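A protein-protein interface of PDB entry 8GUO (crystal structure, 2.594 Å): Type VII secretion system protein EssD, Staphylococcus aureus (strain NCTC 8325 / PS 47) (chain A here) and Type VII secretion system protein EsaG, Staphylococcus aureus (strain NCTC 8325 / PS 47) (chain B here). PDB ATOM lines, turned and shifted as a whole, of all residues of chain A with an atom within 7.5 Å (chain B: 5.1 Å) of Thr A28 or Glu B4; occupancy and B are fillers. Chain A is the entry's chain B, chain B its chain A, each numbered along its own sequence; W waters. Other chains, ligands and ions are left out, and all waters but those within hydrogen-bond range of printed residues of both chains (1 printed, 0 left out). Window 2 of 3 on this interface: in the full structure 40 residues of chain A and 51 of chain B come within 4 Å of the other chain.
Hydrophobic or aromatic side chains of chain B within 4 Å of the printed part of chain A: Phe B3 and Leu B7.
Hydrophobic or aromatic side chains of chain A within 4 Å of the printed part of chain B: Tyr A26, His A32, Tyr A34 and Ile A42.
Among the printed residues, no Asp or Glu carboxylate lies within 4 Å of a Lys or Arg side-chain nitrogen of the other chain.
OE2 of Glu B4 lies within hydrogen-bond range of OH of Tyr A26, 2.9 Å away.
Among the printed residues, merely in contact across the chains: Tyr A34 with Leu B7 (3.3 Å), His A32 with Ser B8 (3.5 Å), Thr A28 with Glu B4 (3.7 Å), Tyr A34 with Glu B4 (3.8 Å) and Ile A42 with Phe B3 (3.8 Å).
N of His A32 sits close to OG1 of Thr A28 (3.2 Å).
N of Tyr A34 lies within hydrogen-bond range of O of Tyr A26 (2.7 Å).
OG1 of Thr A28 lies within hydrogen-bond range of OG1 of Thr A30 (2.8 Å).
Of the printed residues of chain B, Tyr A26 touches Glu B4.
Thr A27 touches none of the printed residues of chain B.
Of the printed residues of chain B, Thr A28 touches Glu B4 (3.7 Å).
Printed residues of chain B within 4 Å of His A32: Ser B8.
Glu B4 touches three residues of chain A.
Of the printed residues of chain A, Leu B7 touches Tyr A34 (3.3 Å).
Of the printed residues of chain A, Ser B8 touches His A32.
The nearest printed residue of chain B that does not touch Thr A28 is Glu B5 (6.7 Å).
Water W1 lies within hydrogen-bond range of OH of Tyr A34 (2.5 Å), O of Glu B4 (2.9 Å) and ND1 of His A32 (2.9 Å).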
ATOM      1  N   LEU A  20     -20.252  17.769  -2.837  1.00  0.00           N
ATOM      2  CA  LEU A  20     -20.606  17.988  -4.235  1.00  0.00           C
ATOM      3  C   LEU A  20     -21.503  19.211  -4.391  1.00  0.00           C
ATOM      4  O   LEU A  20     -22.232  19.340  -5.375  1.00  0.00           O
ATOM      5  CB  LEU A  20     -21.289  16.748  -4.816  1.00  0.00           C
ATOM      6  N   TYR A  26     -17.862  21.433   4.550  1.00  0.00           N
ATOM      7  CA  TYR A  26     -18.641  20.520   5.379  1.00  0.00           C
ATOM      8  C   TYR A  26     -17.786  19.593   6.234  1.00  0.00           C
ATOM      9  O   TYR A  26     -16.696  19.179   5.840  1.00  0.00           O
ATOM     10  CB  TYR A  26     -19.617  19.705   4.519  1.00  0.00           C
ATOM     11  CG  TYR A  26     -19.036  18.651   3.595  1.00  0.00           C
ATOM     12  CD1 TYR A  26     -18.659  18.969   2.297  1.00  0.00           C
ATOM     13  CD2 TYR A  26     -18.924  17.328   4.003  1.00  0.00           C
ATOM     14  CE1 TYR A  26     -18.157  18.004   1.443  1.00  0.00           C
ATOM     15  CE2 TYR A  26     -18.420  16.359   3.157  1.00  0.00           C
ATOM     16  CZ  TYR A  26     -18.039  16.703   1.880  1.00  0.00           C
ATOM     17  OH  TYR A  26     -17.540  15.743   1.034  1.00  0.00           O
ATOM     18  N   THR A  27     -18.307  19.290   7.421  1.00  0.00           N
ATOM     19  CA  THR A  27     -17.612  18.482   8.413  1.00  0.00           C
ATOM     20  C   THR A  27     -18.350  17.166   8.647  1.00  0.00           C
ATOM     21  O   THR A  27     -19.552  17.159   8.910  1.00  0.00           O
ATOM     22  CB  THR A  27     -17.476  19.238   9.748  1.00  0.00           C
ATOM     23  OG1 THR A  27     -16.767  20.466   9.536  1.00  0.00           O
ATOM     24  CG2 THR A  27     -16.739  18.391  10.778  1.00  0.00           C
ATOM     25  N   THR A  28     -17.622  16.060   8.550  1.00  0.00           N
ATOM     26  CA  THR A  28     -18.201  14.729   8.692  1.00  0.00           C
ATOM     27  C   THR A  28     -18.396  14.380  10.167  1.00  0.00           C
ATOM     28  O   THR A  28     -17.856  15.065  11.033  1.00  0.00           O
ATOM     29  CB  THR A  28     -17.308  13.675   8.001  1.00  0.00           C
ATOM     30  OG1 THR A  28     -16.120  13.464   8.772  1.00  0.00           O
ATOM     31  CG2 THR A  28     -16.933  14.145   6.606  1.00  0.00           C
ATOM     32  N   PRO A  29     -19.186  13.327  10.459  1.00  0.00           N
ATOM     33  CA  PRO A  29     -19.344  12.857  11.843  1.00  0.00           C
ATOM     34  C   PRO A  29     -18.028  12.652  12.595  1.00  0.00           C
ATOM     35  O   PRO A  29     -18.001  12.759  13.820  1.00  0.00           O
ATOM     36  CB  PRO A  29     -20.070  11.518  11.671  1.00  0.00           C
ATOM     37  CG  PRO A  29     -20.867  11.686  10.434  1.00  0.00           C
ATOM     38  CD  PRO A  29     -20.108  12.631   9.539  1.00  0.00           C
ATOM     39  N   THR A  30     -16.960  12.371  11.861  1.00  0.00           N
ATOM     40  CA  THR A  30     -15.679  12.014  12.454  1.00  0.00           C
ATOM     41  C   THR A  30     -14.759  13.216  12.632  1.00  0.00           C
ATOM     42  O   THR A  30     -13.627  13.078  13.095  1.00  0.00           O
ATOM     43  CB  THR A  30     -14.980  10.946  11.596  1.00  0.00           C
ATOM     44  OG1 THR A  30     -14.936  11.392  10.235  1.00  0.00           O
ATOM     45  CG2 THR A  30     -15.749   9.646  11.665  1.00  0.00           C
ATOM     46  N   GLY A  31     -15.250  14.394  12.262  1.00  0.00           N
ATOM     47  CA  GLY A  31     -14.491  15.622  12.422  1.00  0.00           C
ATOM     48  C   GLY A  31     -13.779  16.107  11.166  1.00  0.00           C
ATOM     49  O   GLY A  31     -13.129  17.157  11.185  1.00  0.00           O
ATOM     50  N   HIS A  32     -13.913  15.349  10.081  1.00  0.00           N
ATOM     51  CA  HIS A  32     -13.202  15.617   8.839  1.00  0.00           C
ATOM     52  C   HIS A  32     -13.811  16.801   8.099  1.00  0.00           C
ATOM     53  O   HIS A  32     -15.006  16.806   7.818  1.00  0.00           O
ATOM     54  CB  HIS A  32     -13.231  14.369   7.960  1.00  0.00           C
ATOM     55  CG  HIS A  32     -12.409  13.236   8.489  1.00  0.00           C
ATOM     56  ND1 HIS A  32     -11.407  12.627   7.766  1.00  0.00           N
ATOM     57  CD2 HIS A  32     -12.393  12.648   9.712  1.00  0.00           C
ATOM     58  CE1 HIS A  32     -10.847  11.680   8.497  1.00  0.00           C
ATOM     59  NE2 HIS A  32     -11.421  11.680   9.685  1.00  0.00           N
ATOM     60  N   ILE A  33     -12.992  17.801   7.786  1.00  0.00           N
ATOM     61  CA  ILE A  33     -13.479  19.019   7.145  1.00  0.00           C
ATOM     62  C   ILE A  33     -13.176  19.041   5.649  1.00  0.00           C
ATOM     63  O   ILE A  33     -12.036  18.848   5.240  1.00  0.00           O
ATOM     64  CB  ILE A  33     -12.867  20.276   7.798  1.00  0.00           C
ATOM     65  CG1 ILE A  33     -13.060  20.224   9.311  1.00  0.00           C
ATOM     66  CG2 ILE A  33     -13.483  21.540   7.210  1.00  0.00           C
ATOM     67  CD1 ILE A  33     -12.544  21.439  10.037  1.00  0.00           C
ATOM     68  N   TYR A  34     -14.201  19.286   4.837  1.00  0.00           N
ATOM     69  CA  TYR A  34     -14.055  19.290   3.383  1.00  0.00           C
ATOM     70  C   TYR A  34     -14.442  20.638   2.785  1.00  0.00           C
ATOM     71  O   TYR A  34     -15.404  21.258   3.227  1.00  0.00           O
ATOM     72  CB  TYR A  34     -14.910  18.184   2.758  1.00  0.00           C
ATOM     73  CG  TYR A  34     -14.312  16.800   2.850  1.00  0.00           C
ATOM     74  CD1 TYR A  34     -14.392  16.064   4.022  1.00  0.00           C
ATOM     75  CD2 TYR A  34     -13.686  16.221   1.757  1.00  0.00           C
ATOM     76  CE1 TYR A  34     -13.855  14.799   4.109  1.00  0.00           C
ATOM     77  CE2 TYR A  34     -13.144  14.953   1.832  1.00  0.00           C
ATOM     78  CZ  TYR A  34     -13.230  14.249   3.012  1.00  0.00           C
ATOM     79  OH  TYR A  34     -12.693  12.987   3.094  1.00  0.00           O
ATOM     80  N   ILE A  42     -14.153  18.697  -4.527  1.00  0.00           N
ATOM     81  CA  ILE A  42     -13.347  18.758  -3.313  1.00  0.00           C
ATOM     82  C   ILE A  42     -11.965  19.323  -3.630  1.00  0.00           C
ATOM     83  O   ILE A  42     -11.281  18.844  -4.534  1.00  0.00           O
ATOM     84  CB  ILE A  42     -13.194  17.368  -2.657  1.00  0.00           C
ATOM     85  CG1 ILE A  42     -14.559  16.804  -2.265  1.00  0.00           C
ATOM     86  CG2 ILE A  42     -12.291  17.448  -1.435  1.00  0.00           C
ATOM     87  CD1 ILE A  42     -14.568  15.303  -2.078  1.00  0.00           C
ATOM     88  N   VAL A  45      -9.079  19.129   2.292  1.00  0.00           N
ATOM     89  CA  VAL A  45      -9.532  18.233   3.351  1.00  0.00           C
ATOM     90  C   VAL A  45      -8.687  18.442   4.598  1.00  0.00           C
ATOM     91  O   VAL A  45      -7.464  18.510   4.503  1.00  0.00           O
ATOM     92  CB  VAL A  45      -9.439  16.743   2.947  1.00  0.00           C
ATOM     93  CG1 VAL A  45     -10.163  15.876   3.969  1.00  0.00           C
ATOM     94  CG2 VAL A  45     -10.006  16.511   1.562  1.00  0.00           C
ATOM     95  N   TYR A  46      -9.325  18.545   5.761  1.00  0.00           N
ATOM     96  CA  TYR A  46      -8.576  18.602   7.015  1.00  0.00           C
ATOM     97  C   TYR A  46      -8.907  17.425   7.924  1.00  0.00           C
ATOM     98  O   TYR A  46     -10.074  17.096   8.146  1.00  0.00           O
ATOM     99  CB  TYR A  46      -8.824  19.909   7.774  1.00  0.00           C
ATOM    100  CG  TYR A  46      -8.094  19.941   9.104  1.00  0.00           C
ATOM    101  CD1 TYR A  46      -6.721  20.157   9.156  1.00  0.00           C
ATOM    102  CD2 TYR A  46      -8.769  19.734  10.306  1.00  0.00           C
ATOM    103  CE1 TYR A  46      -6.039  20.177  10.364  1.00  0.00           C
ATOM    104  CE2 TYR A  46      -8.091  19.753  11.521  1.00  0.00           C
ATOM    105  CZ  TYR A  46      -6.726  19.975  11.540  1.00  0.00           C
ATOM    106  OH  TYR A  46      -6.041  19.998  12.735  1.00  0.00           O
ATOM    107  N   ASN A  49      -6.999  13.315  12.641  1.00  0.00           N
ATOM    108  CA  ASN A  49      -7.513  12.041  13.126  1.00  0.00           C
ATOM    109  C   ASN A  49      -6.776  10.788  12.636  1.00  0.00           C
ATOM    110  O   ASN A  49      -7.168   9.674  12.976  1.00  0.00           O
ATOM    111  CB  ASN A  49      -8.995  11.945  12.743  1.00  0.00           C
ATOM    112  CG  ASN A  49      -9.797  11.098  13.702  1.00  0.00           C
ATOM    113  OD1 ASN A  49      -9.304  10.693  14.755  1.00  0.00           O
ATOM    114  ND2 ASN A  49     -11.051  10.838  13.351  1.00  0.00           N
ATOM    115  N   THR B   2     -19.715   5.296   4.011  1.00  0.00           N
ATOM    116  CA  THR B   2     -19.922   6.548   3.295  1.00  0.00           C
ATOM    117  C   THR B   2     -18.709   6.866   2.419  1.00  0.00           C
ATOM    118  O   THR B   2     -17.670   6.210   2.516  1.00  0.00           O
ATOM    119  CB  THR B   2     -20.178   7.719   4.262  1.00  0.00           C
ATOM    120  OG1 THR B   2     -19.022   7.932   5.081  1.00  0.00           O
ATOM    121  CG2 THR B   2     -21.381   7.431   5.155  1.00  0.00           C
ATOM    122  N   PHE B   3     -18.848   7.870   1.560  1.00  0.00           N
ATOM    123  CA  PHE B   3     -17.755   8.286   0.690  1.00  0.00           C
ATOM    124  C   PHE B   3     -16.548   8.760   1.490  1.00  0.00           C
ATOM    125  O   PHE B   3     -15.405   8.442   1.158  1.00  0.00           O
ATOM    126  CB  PHE B   3     -18.229   9.385  -0.264  1.00  0.00           C
ATOM    127  CG  PHE B   3     -17.144   9.934  -1.144  1.00  0.00           C
ATOM    128  CD1 PHE B   3     -16.212   9.092  -1.730  1.00  0.00           C
ATOM    129  CD2 PHE B   3     -17.063  11.293  -1.393  1.00  0.00           C
ATOM    130  CE1 PHE B   3     -15.217   9.598  -2.538  1.00  0.00           C
ATOM    131  CE2 PHE B   3     -16.072  11.804  -2.202  1.00  0.00           C
ATOM    132  CZ  PHE B   3     -15.147  10.955  -2.776  1.00  0.00           C
ATOM    133  N   GLU B   4     -16.810   9.510   2.553  1.00  0.00           N
ATOM    134  CA  GLU B   4     -15.753  10.086   3.371  1.00  0.00           C
ATOM    135  C   GLU B   4     -15.098   9.044   4.269  1.00  0.00           C
ATOM    136  O   GLU B   4     -13.978   9.238   4.742  1.00  0.00           O
ATOM    137  CB  GLU B   4     -16.307  11.241   4.209  1.00  0.00           C
ATOM    138  CG  GLU B   4     -16.729  12.442   3.381  1.00  0.00           C
ATOM    139  CD  GLU B   4     -18.115  12.293   2.778  1.00  0.00           C
ATOM    140  OE1 GLU B   4     -18.843  11.358   3.171  1.00  0.00           O
ATOM    141  OE2 GLU B   4     -18.475  13.107   1.903  1.00  0.00           O
ATOM    142  N   GLU B   5     -15.798   7.938   4.501  1.00  0.00           N
ATOM    143  CA  GLU B   5     -15.236   6.837   5.271  1.00  0.00           C
ATOM    144  C   GLU B   5     -14.287   6.020   4.396  1.00  0.00           C
ATOM    145  O   GLU B   5     -13.301   5.470   4.881  1.00  0.00           O
ATOM    146  CB  GLU B   5     -16.347   5.952   5.849  1.00  0.00           C
ATOM    147  CG  GLU B   5     -16.971   6.496   7.132  1.00  0.00           C
ATOM    148  CD  GLU B   5     -18.186   5.705   7.586  1.00  0.00           C
ATOM    149  OE1 GLU B   5     -18.880   5.132   6.721  1.00  0.00           O
ATOM    150  OE2 GLU B   5     -18.449   5.659   8.807  1.00  0.00           O
ATOM    151  N   LYS B   6     -14.584   5.956   3.104  1.00  0.00           N
ATOM    152  CA  LYS B   6     -13.707   5.283   2.152  1.00  0.00           C
ATOM    153  C   LYS B   6     -12.434   6.097   1.945  1.00  0.00           C
ATOM    154  O   LYS B   6     -11.334   5.544   1.877  1.00  0.00           O
ATOM    155  CB  LYS B   6     -14.422   5.066   0.817  1.00  0.00           C
ATOM    156  CG  LYS B   6     -15.631   4.146   0.894  1.00  0.00           C
ATOM    157  CD  LYS B   6     -16.396   4.139  -0.422  1.00  0.00           C
ATOM    158  CE  LYS B   6     -17.609   3.221  -0.358  1.00  0.00           C
ATOM    159  NZ  LYS B   6     -18.573   3.490  -1.467  1.00  0.00           N
ATOM    160  N   LEU B   7     -12.597   7.413   1.850  1.00  0.00           N
ATOM    161  CA  LEU B   7     -11.469   8.327   1.709  1.00  0.00           C
ATOM    162  C   LEU B   7     -10.572   8.274   2.939  1.00  0.00           C
ATOM    163  O   LEU B   7      -9.352   8.341   2.826  1.00  0.00           O
ATOM    164  CB  LEU B   7     -11.959   9.760   1.479  1.00  0.00           C
ATOM    165  CG  LEU B   7     -12.691  10.063   0.170  1.00  0.00           C
ATOM    166  CD1 LEU B   7     -13.115  11.524   0.126  1.00  0.00           C
ATOM    167  CD2 LEU B   7     -11.827   9.717  -1.029  1.00  0.00           C
ATOM    168  N   SER B   8     -11.180   8.148   4.114  1.00  0.00           N
ATOM    169  CA  SER B   8     -10.418   8.085   5.356  1.00  0.00           C
ATOM    170  C   SER B   8      -9.602   6.799   5.425  1.00  0.00           C
ATOM    171  O   SER B   8      -8.457   6.806   5.878  1.00  0.00           O
ATOM    172  CB  SER B   8     -11.347   8.194   6.565  1.00  0.00           C
ATOM    173  OG  SER B   8     -10.599   8.304   7.761  1.00  0.00           O
HETATM  174  O   HOH W   1     -12.779  11.831   5.302  1.00  0.00           O
